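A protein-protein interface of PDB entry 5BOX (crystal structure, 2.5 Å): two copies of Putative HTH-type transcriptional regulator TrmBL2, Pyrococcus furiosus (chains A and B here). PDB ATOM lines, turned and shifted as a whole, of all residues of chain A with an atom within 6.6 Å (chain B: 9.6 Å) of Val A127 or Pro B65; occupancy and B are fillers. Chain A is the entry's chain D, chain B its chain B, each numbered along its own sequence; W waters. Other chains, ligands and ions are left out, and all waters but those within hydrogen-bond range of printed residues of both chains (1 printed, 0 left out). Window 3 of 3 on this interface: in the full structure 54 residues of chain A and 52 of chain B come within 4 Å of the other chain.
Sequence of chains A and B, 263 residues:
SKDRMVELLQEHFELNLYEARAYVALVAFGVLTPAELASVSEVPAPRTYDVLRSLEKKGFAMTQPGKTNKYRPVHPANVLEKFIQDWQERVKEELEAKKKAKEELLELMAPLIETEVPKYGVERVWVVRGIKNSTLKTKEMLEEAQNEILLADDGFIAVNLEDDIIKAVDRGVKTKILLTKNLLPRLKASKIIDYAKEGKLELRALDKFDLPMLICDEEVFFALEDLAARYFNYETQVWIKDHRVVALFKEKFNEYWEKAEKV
The side-chain carboxylate (OE2) of Glu B56 lies within salt-bridge range of the guanidinium group (NH2) of Arg A129 (3.2 Å). The backbone carbonyl oxygen (O) of Thr B63 sits at hydrogen-bond distance from the backbone NH (N) of Val A127, 2.8 Å away. O of Val A125 sits close to NE2 of Gln B64 (2.4 Å).
The backbone NH of Met B62 lies within hydrogen-bond range of the backbone carbonyl oxygen of Arg B72. The side-chain hydroxyl (OG1) of Thr B63 lies within hydrogen-bond range of the backbone carbonyl oxygen (O) of Lys B70 (3.5 Å). The backbone NH (N) of Gln B64 is in hydrogen-bond range of the backbone carbonyl oxygen (O) of Lys B70 (2.9 Å). O of Trp A126 is in hydrogen-bond range of N of Trp A239 (2.9 Å). The backbone carbonyl oxygen (O) of Gln A237 sits at hydrogen-bond distance from the backbone NH (N) of Val A128 (2.9 Å). The guanidinium group (NH1) of Arg A129 is in hydrogen-bond range of the side-chain hydroxyl (OG1) of Thr A236, 2.7 Å away.
Among the printed residues, pairs that only touch across the chains: Trp A126 with Thr B63 (3.6 Å), Trp A126 with Gln B64 (3.6 Å), Trp A126 with Lys B70 (3.7 Å), Trp A126 with Arg B72 (3.5 Å), Val A127 with Met B62 (3.5 Å), Val A127 with Pro B65 (3.7 Å) and Val A128 with Met B62 (3.7 Å).
Val A127 touches three residues of chain B. Printed residues of chain B within 4 Å of Val A128: Met B62 (3.7 Å). Lys B57 touches none of the printed residues of chain A. Printed residues of chain A within 4 Å of Thr B63: Trp A126 (3.6 Å) and Val A127 (2.8 Å). Of chain A, only Val A127 (3.7 Å) comes within 4 Å of Pro B65. Printed residues of chain A within 4 Å of Lys B70: Trp A126. The nearest printed residue of chain B that does not touch Val A127 is Gln B64 (5.0 Å). The nearest residue of chain A that does not touch Pro B65 is Arg A129 (4.3 Å). The nearest printed residue of chain A that does not touch Arg B72 is Trp A239 (6.4 Å).
Of the 10 printed residues of chain A, 5 touch a printed residue of chain B. Along chain A the printed residues that touch a printed residue of chain B span positions 125 to 129. Of the 20 printed residues of chain B, 7 touch a printed residue of chain A. Printed residues of chain B that touch a printed residue of chain A: Glu B56, Met B62, Thr B63, Gln B64, Pro B65, Lys B70 and Arg B72. Along chain B the printed residues that touch a printed residue of chain A span positions 56 to 72. Among the printed residues, Asp or Glu carboxylates within 4 Å of a Lys or Arg side-chain nitrogen of the other chain: Arg A129 with Glu B56.
No position is printed for both chains.
Water W1 bridges NH1 of Arg B72 (3.3 Å) and NE1 of Trp A126 (3.5 Å).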
ATOM      1  N   VAL A 125      15.773 -20.356  -0.850  1.00  0.00           N
ATOM      2  CA  VAL A 125      14.803 -21.442  -0.915  1.00  0.00           C
ATOM      3  C   VAL A 125      13.895 -21.285  -2.130  1.00  0.00           C
ATOM      4  O   VAL A 125      13.316 -20.223  -2.355  1.00  0.00           O
ATOM      5  CB  VAL A 125      13.973 -21.529   0.382  1.00  0.00           C
ATOM      6  CG1 VAL A 125      13.239 -20.221   0.630  1.00  0.00           C
ATOM      7  CG2 VAL A 125      13.003 -22.707   0.324  1.00  0.00           C
ATOM      8  N   TRP A 126      13.808 -22.338  -2.932  1.00  0.00           N
ATOM      9  CA  TRP A 126      12.899 -22.356  -4.074  1.00  0.00           C
ATOM     10  C   TRP A 126      12.172 -23.684  -4.152  1.00  0.00           C
ATOM     11  O   TRP A 126      12.692 -24.718  -3.723  1.00  0.00           O
ATOM     12  CB  TRP A 126      13.640 -22.111  -5.386  1.00  0.00           C
ATOM     13  CG  TRP A 126      14.148 -20.714  -5.566  1.00  0.00           C
ATOM     14  CD1 TRP A 126      15.446 -20.298  -5.498  1.00  0.00           C
ATOM     15  CD2 TRP A 126      13.366 -19.546  -5.852  1.00  0.00           C
ATOM     16  NE1 TRP A 126      15.523 -18.946  -5.735  1.00  0.00           N
ATOM     17  CE2 TRP A 126      14.261 -18.460  -5.953  1.00  0.00           C
ATOM     18  CE3 TRP A 126      11.999 -19.314  -6.031  1.00  0.00           C
ATOM     19  CZ2 TRP A 126      13.829 -17.161  -6.226  1.00  0.00           C
ATOM     20  CZ3 TRP A 126      11.573 -18.020  -6.305  1.00  0.00           C
ATOM     21  CH2 TRP A 126      12.484 -16.963  -6.401  1.00  0.00           C
ATOM     22  N   VAL A 127      10.960 -23.650  -4.690  1.00  0.00           N
ATOM     23  CA  VAL A 127      10.191 -24.864  -4.894  1.00  0.00           C
ATOM     24  C   VAL A 127      10.083 -25.160  -6.387  1.00  0.00           C
ATOM     25  O   VAL A 127       9.973 -24.239  -7.209  1.00  0.00           O
ATOM     26  CB  VAL A 127       8.813 -24.746  -4.233  1.00  0.00           C
ATOM     27  CG1 VAL A 127       7.919 -25.898  -4.648  1.00  0.00           C
ATOM     28  CG2 VAL A 127       8.965 -24.685  -2.716  1.00  0.00           C
ATOM     29  N   VAL A 128      10.109 -26.450  -6.723  1.00  0.00           N
ATOM     30  CA  VAL A 128       9.993 -26.915  -8.102  1.00  0.00           C
ATOM     31  C   VAL A 128       8.907 -27.995  -8.205  1.00  0.00           C
ATOM     32  O   VAL A 128       8.927 -28.967  -7.448  1.00  0.00           O
ATOM     33  CB  VAL A 128      11.349 -27.438  -8.616  1.00  0.00           C
ATOM     34  CG1 VAL A 128      11.189 -28.150  -9.951  1.00  0.00           C
ATOM     35  CG2 VAL A 128      12.351 -26.290  -8.737  1.00  0.00           C
ATOM     36  N   ARG A 129       7.958 -27.810  -9.127  1.00  0.00           N
ATOM     37  CA  ARG A 129       6.826 -28.733  -9.298  1.00  0.00           C
ATOM     38  C   ARG A 129       7.088 -29.857 -10.301  1.00  0.00           C
ATOM     39  O   ARG A 129       7.518 -29.609 -11.429  1.00  0.00           O
ATOM     40  CB  ARG A 129       5.574 -27.986  -9.759  1.00  0.00           C
ATOM     41  CG  ARG A 129       5.170 -26.831  -8.890  1.00  0.00           C
ATOM     42  CD  ARG A 129       4.627 -27.287  -7.557  1.00  0.00           C
ATOM     43  NE  ARG A 129       4.208 -26.136  -6.764  1.00  0.00           N
ATOM     44  CZ  ARG A 129       3.772 -26.205  -5.515  1.00  0.00           C
ATOM     45  NH1 ARG A 129       3.717 -27.375  -4.894  1.00  0.00           N
ATOM     46  NH2 ARG A 129       3.415 -25.099  -4.879  1.00  0.00           N
ATOM     47  N   GLU A 235       4.264 -33.158  -7.814  1.00  0.00           N
ATOM     48  CA  GLU A 235       5.043 -33.426  -6.610  1.00  0.00           C
ATOM     49  C   GLU A 235       5.898 -32.223  -6.267  1.00  0.00           C
ATOM     50  O   GLU A 235       6.431 -31.557  -7.155  1.00  0.00           O
ATOM     51  CB  GLU A 235       5.932 -34.658  -6.787  1.00  0.00           C
ATOM     52  CG  GLU A 235       6.693 -35.044  -5.528  1.00  0.00           C
ATOM     53  CD  GLU A 235       5.767 -35.245  -4.350  1.00  0.00           C
ATOM     54  OE1 GLU A 235       5.210 -36.359  -4.214  1.00  0.00           O
ATOM     55  OE2 GLU A 235       5.584 -34.285  -3.569  1.00  0.00           O
ATOM     56  N   THR A 236       6.027 -31.936  -4.977  1.00  0.00           N
ATOM     57  CA  THR A 236       6.810 -30.786  -4.554  1.00  0.00           C
ATOM     58  C   THR A 236       8.249 -31.156  -4.254  1.00  0.00           C
ATOM     59  O   THR A 236       8.526 -32.078  -3.483  1.00  0.00           O
ATOM     60  CB  THR A 236       6.206 -30.109  -3.326  1.00  0.00           C
ATOM     61  OG1 THR A 236       5.052 -29.363  -3.723  1.00  0.00           O
ATOM     62  CG2 THR A 236       7.225 -29.180  -2.681  1.00  0.00           C
ATOM     63  N   GLN A 237       9.157 -30.424  -4.889  1.00  0.00           N
ATOM     64  CA  GLN A 237      10.584 -30.555  -4.644  1.00  0.00           C
ATOM     65  C   GLN A 237      11.115 -29.245  -4.081  1.00  0.00           C
ATOM     66  O   GLN A 237      10.665 -28.164  -4.472  1.00  0.00           O
ATOM     67  CB  GLN A 237      11.312 -30.929  -5.933  1.00  0.00           C
ATOM     68  CG  GLN A 237      11.031 -32.342  -6.402  1.00  0.00           C
ATOM     69  CD  GLN A 237      11.159 -32.488  -7.904  1.00  0.00           C
ATOM     70  OE1 GLN A 237      11.792 -33.422  -8.397  1.00  0.00           O
ATOM     71  NE2 GLN A 237      10.543 -31.573  -8.643  1.00  0.00           N
ATOM     72  N   VAL A 238      12.068 -29.345  -3.159  1.00  0.00           N
ATOM     73  CA  VAL A 238      12.580 -28.172  -2.459  1.00  0.00           C
ATOM     74  C   VAL A 238      14.081 -28.004  -2.636  1.00  0.00           C
ATOM     75  O   VAL A 238      14.837 -28.979  -2.588  1.00  0.00           O
ATOM     76  CB  VAL A 238      12.256 -28.231  -0.958  1.00  0.00           C
ATOM     77  CG1 VAL A 238      12.726 -26.955  -0.274  1.00  0.00           C
ATOM     78  CG2 VAL A 238      10.781 -28.467  -0.734  1.00  0.00           C
ATOM     79  N   TRP A 239      14.505 -26.756  -2.823  1.00  0.00           N
ATOM     80  CA  TRP A 239      15.920 -26.396  -2.843  1.00  0.00           C
ATOM     81  C   TRP A 239      16.252 -25.446  -1.700  1.00  0.00           C
ATOM     82  O   TRP A 239      15.713 -24.340  -1.635  1.00  0.00           O
ATOM     83  CB  TRP A 239      16.303 -25.751  -4.173  1.00  0.00           C
ATOM     84  CG  TRP A 239      17.680 -25.155  -4.175  1.00  0.00           C
ATOM     85  CD1 TRP A 239      18.859 -25.815  -4.357  1.00  0.00           C
ATOM     86  CD2 TRP A 239      18.019 -23.772  -4.004  1.00  0.00           C
ATOM     87  NE1 TRP A 239      19.912 -24.933  -4.307  1.00  0.00           N
ATOM     88  CE2 TRP A 239      19.423 -23.672  -4.091  1.00  0.00           C
ATOM     89  CE3 TRP A 239      17.273 -22.610  -3.784  1.00  0.00           C
ATOM     90  CZ2 TRP A 239      20.093 -22.458  -3.965  1.00  0.00           C
ATOM     91  CZ3 TRP A 239      17.944 -21.405  -3.660  1.00  0.00           C
ATOM     92  CH2 TRP A 239      19.337 -21.338  -3.750  1.00  0.00           C
ATOM     93  N   ARG B  53       1.314 -19.421 -12.028  1.00  0.00           N
ATOM     94  CA  ARG B  53       1.144 -20.759 -11.480  1.00  0.00           C
ATOM     95  C   ARG B  53       1.156 -21.767 -12.632  1.00  0.00           C
ATOM     96  O   ARG B  53       1.507 -22.937 -12.450  1.00  0.00           O
ATOM     97  CB  ARG B  53      -0.147 -20.856 -10.658  1.00  0.00           C
ATOM     98  CG  ARG B  53      -0.098 -21.891  -9.537  1.00  0.00           C
ATOM     99  CD  ARG B  53      -0.166 -21.236  -8.160  1.00  0.00           C
ATOM    100  NE  ARG B  53      -1.249 -20.259  -8.075  1.00  0.00           N
ATOM    101  CZ  ARG B  53      -1.562 -19.574  -6.979  1.00  0.00           C
ATOM    102  NH1 ARG B  53      -0.877 -19.761  -5.858  1.00  0.00           N
ATOM    103  NH2 ARG B  53      -2.563 -18.701  -7.001  1.00  0.00           N
ATOM    104  N   LEU B  55       3.070 -21.364 -15.494  1.00  0.00           N
ATOM    105  CA  LEU B  55       4.491 -21.512 -15.820  1.00  0.00           C
ATOM    106  C   LEU B  55       5.179 -22.424 -14.806  1.00  0.00           C
ATOM    107  O   LEU B  55       6.142 -23.128 -15.124  1.00  0.00           O
ATOM    108  CB  LEU B  55       5.189 -20.148 -15.865  1.00  0.00           C
ATOM    109  CG  LEU B  55       4.776 -19.183 -16.982  1.00  0.00           C
ATOM    110  CD1 LEU B  55       5.531 -17.852 -16.899  1.00  0.00           C
ATOM    111  CD2 LEU B  55       4.988 -19.826 -18.348  1.00  0.00           C
ATOM    112  N   GLU B  56       4.657 -22.424 -13.587  1.00  0.00           N
ATOM    113  CA  GLU B  56       5.203 -23.243 -12.520  1.00  0.00           C
ATOM    114  C   GLU B  56       5.185 -24.726 -12.896  1.00  0.00           C
ATOM    115  O   GLU B  56       6.233 -25.371 -12.918  1.00  0.00           O
ATOM    116  CB  GLU B  56       4.418 -22.991 -11.229  1.00  0.00           C
ATOM    117  CG  GLU B  56       4.901 -23.753 -10.009  1.00  0.00           C
ATOM    118  CD  GLU B  56       4.125 -23.376  -8.760  1.00  0.00           C
ATOM    119  OE1 GLU B  56       3.652 -22.222  -8.686  1.00  0.00           O
ATOM    120  OE2 GLU B  56       3.984 -24.225  -7.856  1.00  0.00           O
ATOM    121  N   LYS B  57       4.012 -25.253 -13.240  1.00  0.00           N
ATOM    122  CA  LYS B  57       3.874 -26.681 -13.543  1.00  0.00           C
ATOM    123  C   LYS B  57       4.564 -27.079 -14.854  1.00  0.00           C
ATOM    124  O   LYS B  57       5.078 -28.193 -14.977  1.00  0.00           O
ATOM    125  CB  LYS B  57       2.393 -27.069 -13.602  1.00  0.00           C
ATOM    126  CG  LYS B  57       2.124 -28.574 -13.493  1.00  0.00           C
ATOM    127  CD  LYS B  57       0.623 -28.875 -13.527  1.00  0.00           C
ATOM    128  CE  LYS B  57       0.343 -30.372 -13.442  1.00  0.00           C
ATOM    129  NZ  LYS B  57      -1.092 -30.695 -13.715  1.00  0.00           N
ATOM    130  N   GLY B  59       7.274 -25.966 -15.995  1.00  0.00           N
ATOM    131  CA  GLY B  59       8.710 -26.013 -15.786  1.00  0.00           C
ATOM    132  C   GLY B  59       9.474 -24.774 -16.213  1.00  0.00           C
ATOM    133  O   GLY B  59      10.697 -24.810 -16.349  1.00  0.00           O
ATOM    134  N   PHE B  60       8.763 -23.669 -16.404  1.00  0.00           N
ATOM    135  CA  PHE B  60       9.391 -22.431 -16.847  1.00  0.00           C
ATOM    136  C   PHE B  60       9.675 -21.519 -15.674  1.00  0.00           C
ATOM    137  O   PHE B  60      10.298 -20.464 -15.824  1.00  0.00           O
ATOM    138  CB  PHE B  60       8.504 -21.722 -17.868  1.00  0.00           C
ATOM    139  CG  PHE B  60       8.507 -22.378 -19.214  1.00  0.00           C
ATOM    140  CD1 PHE B  60       7.898 -23.610 -19.400  1.00  0.00           C
ATOM    141  CD2 PHE B  60       9.123 -21.771 -20.292  1.00  0.00           C
ATOM    142  CE1 PHE B  60       7.912 -24.221 -20.637  1.00  0.00           C
ATOM    143  CE2 PHE B  60       9.134 -22.377 -21.537  1.00  0.00           C
ATOM    144  CZ  PHE B  60       8.530 -23.600 -21.709  1.00  0.00           C
ATOM    145  N   ALA B  61       9.246 -21.949 -14.493  1.00  0.00           N
ATOM    146  CA  ALA B  61       9.364 -21.117 -13.310  1.00  0.00           C
ATOM    147  C   ALA B  61       9.491 -21.938 -12.035  1.00  0.00           C
ATOM    148  O   ALA B  61       8.913 -23.019 -11.915  1.00  0.00           O
ATOM    149  CB  ALA B  61       8.168 -20.183 -13.214  1.00  0.00           C
ATOM    150  N   MET B  62      10.282 -21.409 -11.103  1.00  0.00           N
ATOM    151  CA  MET B  62      10.357 -21.911  -9.739  1.00  0.00           C
ATOM    152  C   MET B  62       9.639 -20.910  -8.843  1.00  0.00           C
ATOM    153  O   MET B  62       9.443 -19.751  -9.231  1.00  0.00           O
ATOM    154  CB  MET B  62      11.802 -22.096  -9.288  1.00  0.00           C
ATOM    155  CG  MET B  62      12.649 -22.940 -10.219  1.00  0.00           C
ATOM    156  SD  MET B  62      14.341 -23.083  -9.614  1.00  0.00           S
ATOM    157  CE  MET B  62      15.109 -23.978 -10.962  1.00  0.00           C
ATOM    158  N   THR B  63       9.243 -21.336  -7.651  1.00  0.00           N
ATOM    159  CA  THR B  63       8.394 -20.471  -6.842  1.00  0.00           C
ATOM    160  C   THR B  63       8.691 -20.519  -5.338  1.00  0.00           C
ATOM    161  O   THR B  63       9.225 -21.506  -4.820  1.00  0.00           O
ATOM    162  CB  THR B  63       6.903 -20.828  -7.069  1.00  0.00           C
ATOM    163  OG1 THR B  63       6.070 -19.833  -6.471  1.00  0.00           O
ATOM    164  CG2 THR B  63       6.581 -22.171  -6.449  1.00  0.00           C
ATOM    165  N   GLN B  64       8.353 -19.433  -4.649  1.00  0.00           N
ATOM    166  CA  GLN B  64       8.335 -19.422  -3.191  1.00  0.00           C
ATOM    167  C   GLN B  64       6.910 -19.238  -2.680  1.00  0.00           C
ATOM    168  O   GLN B  64       6.346 -18.146  -2.766  1.00  0.00           O
ATOM    169  CB  GLN B  64       9.246 -18.334  -2.629  1.00  0.00           C
ATOM    170  CG  GLN B  64      10.721 -18.647  -2.718  1.00  0.00           C
ATOM    171  CD  GLN B  64      11.556 -17.672  -1.929  1.00  0.00           C
ATOM    172  OE1 GLN B  64      11.187 -16.510  -1.781  1.00  0.00           O
ATOM    173  NE2 GLN B  64      12.678 -18.142  -1.399  1.00  0.00           N
ATOM    174  N   PRO B  65       6.305 -20.326  -2.195  1.00  0.00           N
ATOM    175  CA  PRO B  65       4.955 -20.328  -1.623  1.00  0.00           C
ATOM    176  C   PRO B  65       4.840 -19.522  -0.332  1.00  0.00           C
ATOM    177  O   PRO B  65       5.391 -19.924   0.691  1.00  0.00           O
ATOM    178  CB  PRO B  65       4.698 -21.811  -1.352  1.00  0.00           C
ATOM    179  CG  PRO B  65       5.598 -22.527  -2.293  1.00  0.00           C
ATOM    180  CD  PRO B  65       6.834 -21.689  -2.358  1.00  0.00           C
ATOM    181  N   GLY B  66       4.091 -18.425  -0.373  1.00  0.00           N
ATOM    182  CA  GLY B  66       3.882 -17.597   0.801  1.00  0.00           C
ATOM    183  C   GLY B  66       2.640 -16.731   0.708  1.00  0.00           C
ATOM    184  O   GLY B  66       1.837 -16.893  -0.210  1.00  0.00           O
ATOM    185  N   LYS B  67       2.473 -15.817   1.658  1.00  0.00           N
ATOM    186  CA  LYS B  67       1.329 -14.912   1.631  1.00  0.00           C
ATOM    187  C   LYS B  67       1.284 -14.182   0.291  1.00  0.00           C
ATOM    188  O   LYS B  67       0.208 -13.900  -0.242  1.00  0.00           O
ATOM    189  CB  LYS B  67       1.389 -13.916   2.789  1.00  0.00           C
ATOM    190  CG  LYS B  67       0.145 -13.047   2.914  1.00  0.00           C
ATOM    191  CD  LYS B  67       0.072 -12.361   4.269  1.00  0.00           C
ATOM    192  CE  LYS B  67       1.248 -11.423   4.488  1.00  0.00           C
ATOM    193  NZ  LYS B  67       1.224 -10.819   5.852  1.00  0.00           N
ATOM    194  N   THR B  68       2.460 -13.882  -0.250  1.00  0.00           N
ATOM    195  CA  THR B  68       2.577 -13.354  -1.604  1.00  0.00           C
ATOM    196  C   THR B  68       3.671 -14.100  -2.358  1.00  0.00           C
ATOM    197  O   THR B  68       4.859 -13.850  -2.158  1.00  0.00           O
ATOM    198  CB  THR B  68       2.884 -11.850  -1.608  1.00  0.00           C
ATOM    199  OG1 THR B  68       4.028 -11.593  -0.783  1.00  0.00           O
ATOM    200  CG2 THR B  68       1.688 -11.065  -1.087  1.00  0.00           C
ATOM    201  N   ASN B  69       3.264 -15.024  -3.220  1.00  0.00           N
ATOM    202  CA  ASN B  69       4.209 -15.849  -3.957  1.00  0.00           C
ATOM    203  C   ASN B  69       5.108 -15.033  -4.876  1.00  0.00           C
ATOM    204  O   ASN B  69       4.645 -14.153  -5.603  1.00  0.00           O
ATOM    205  CB  ASN B  69       3.464 -16.905  -4.776  1.00  0.00           C
ATOM    206  CG  ASN B  69       2.781 -17.935  -3.907  1.00  0.00           C
ATOM    207  OD1 ASN B  69       2.412 -17.655  -2.766  1.00  0.00           O
ATOM    208  ND2 ASN B  69       2.623 -19.141  -4.435  1.00  0.00           N
ATOM    209  N   LYS B  70       6.400 -15.329  -4.834  1.00  0.00           N
ATOM    210  CA  LYS B  70       7.330 -14.743  -5.782  1.00  0.00           C
ATOM    211  C   LYS B  70       7.888 -15.857  -6.671  1.00  0.00           C
ATOM    212  O   LYS B  70       8.050 -17.002  -6.229  1.00  0.00           O
ATOM    213  CB  LYS B  70       8.450 -13.980  -5.069  1.00  0.00           C
ATOM    214  CG  LYS B  70       9.307 -14.821  -4.155  1.00  0.00           C
ATOM    215  CD  LYS B  70      10.554 -14.061  -3.736  1.00  0.00           C
ATOM    216  CE  LYS B  70      10.214 -12.789  -2.985  1.00  0.00           C
ATOM    217  NZ  LYS B  70      11.450 -12.096  -2.529  1.00  0.00           N
ATOM    218  N   TYR B  71       8.174 -15.517  -7.924  1.00  0.00           N
ATOM    219  CA  TYR B  71       8.582 -16.506  -8.912  1.00  0.00           C
ATOM    220  C   TYR B  71       9.912 -16.166  -9.581  1.00  0.00           C
ATOM    221  O   TYR B  71      10.184 -15.004  -9.884  1.00  0.00           O
ATOM    222  CB  TYR B  71       7.497 -16.642  -9.982  1.00  0.00           C
ATOM    223  CG  TYR B  71       6.143 -17.066  -9.450  1.00  0.00           C
ATOM    224  CD1 TYR B  71       5.839 -18.410  -9.267  1.00  0.00           C
ATOM    225  CD2 TYR B  71       5.169 -16.127  -9.143  1.00  0.00           C
ATOM    226  CE1 TYR B  71       4.605 -18.807  -8.792  1.00  0.00           C
ATOM    227  CE2 TYR B  71       3.929 -16.515  -8.665  1.00  0.00           C
ATOM    228  CZ  TYR B  71       3.650 -17.858  -8.489  1.00  0.00           C
ATOM    229  OH  TYR B  71       2.415 -18.256  -8.009  1.00  0.00           O
ATOM    230  N   ARG B  72      10.736 -17.184  -9.816  1.00  0.00           N
ATOM    231  CA  ARG B  72      11.938 -17.010 -10.631  1.00  0.00           C
ATOM    232  C   ARG B  72      11.858 -17.867 -11.890  1.00  0.00           C
ATOM    233  O   ARG B  72      11.388 -19.011 -11.852  1.00  0.00           O
ATOM    234  CB  ARG B  72      13.200 -17.377  -9.850  1.00  0.00           C
ATOM    235  CG  ARG B  72      13.210 -18.823  -9.382  1.00  0.00           C
ATOM    236  CD  ARG B  72      14.613 -19.412  -9.341  1.00  0.00           C
ATOM    237  NE  ARG B  72      15.196 -19.572 -10.670  1.00  0.00           N
ATOM    238  CZ  ARG B  72      16.305 -20.266 -10.923  1.00  0.00           C
ATOM    239  NH1 ARG B  72      16.949 -20.883  -9.933  1.00  0.00           N
ATOM    240  NH2 ARG B  72      16.760 -20.360 -12.169  1.00  0.00           N
ATOM    241  N   PRO B  73      12.356 -17.331 -13.008  1.00  0.00           N
ATOM    242  CA  PRO B  73      12.366 -18.107 -14.246  1.00  0.00           C
ATOM    243  C   PRO B  73      13.392 -19.217 -14.169  1.00  0.00           C
ATOM    244  O   PRO B  73      14.446 -19.038 -13.549  1.00  0.00           O
ATOM    245  CB  PRO B  73      12.761 -17.076 -15.305  1.00  0.00           C
ATOM    246  CG  PRO B  73      13.604 -16.099 -14.553  1.00  0.00           C
ATOM    247  CD  PRO B  73      12.980 -16.007 -13.182  1.00  0.00           C
ATOM    248  N   VAL B  74      13.052 -20.372 -14.727  1.00  0.00           N
ATOM    249  CA  VAL B  74      14.043 -21.405 -14.978  1.00  0.00           C
ATOM    250  C   VAL B  74      14.907 -20.883 -16.121  1.00  0.00           C
ATOM    251  O   VAL B  74      14.459 -20.035 -16.896  1.00  0.00           O
ATOM    252  CB  VAL B  74      13.394 -22.763 -15.302  1.00  0.00           C
ATOM    253  CG1 VAL B  74      14.447 -23.774 -15.721  1.00  0.00           C
ATOM    254  CG2 VAL B  74      12.653 -23.278 -14.089  1.00  0.00           C
HETATM  255  O   HOH W   1      18.488 -20.140  -7.136  1.00  0.00           O
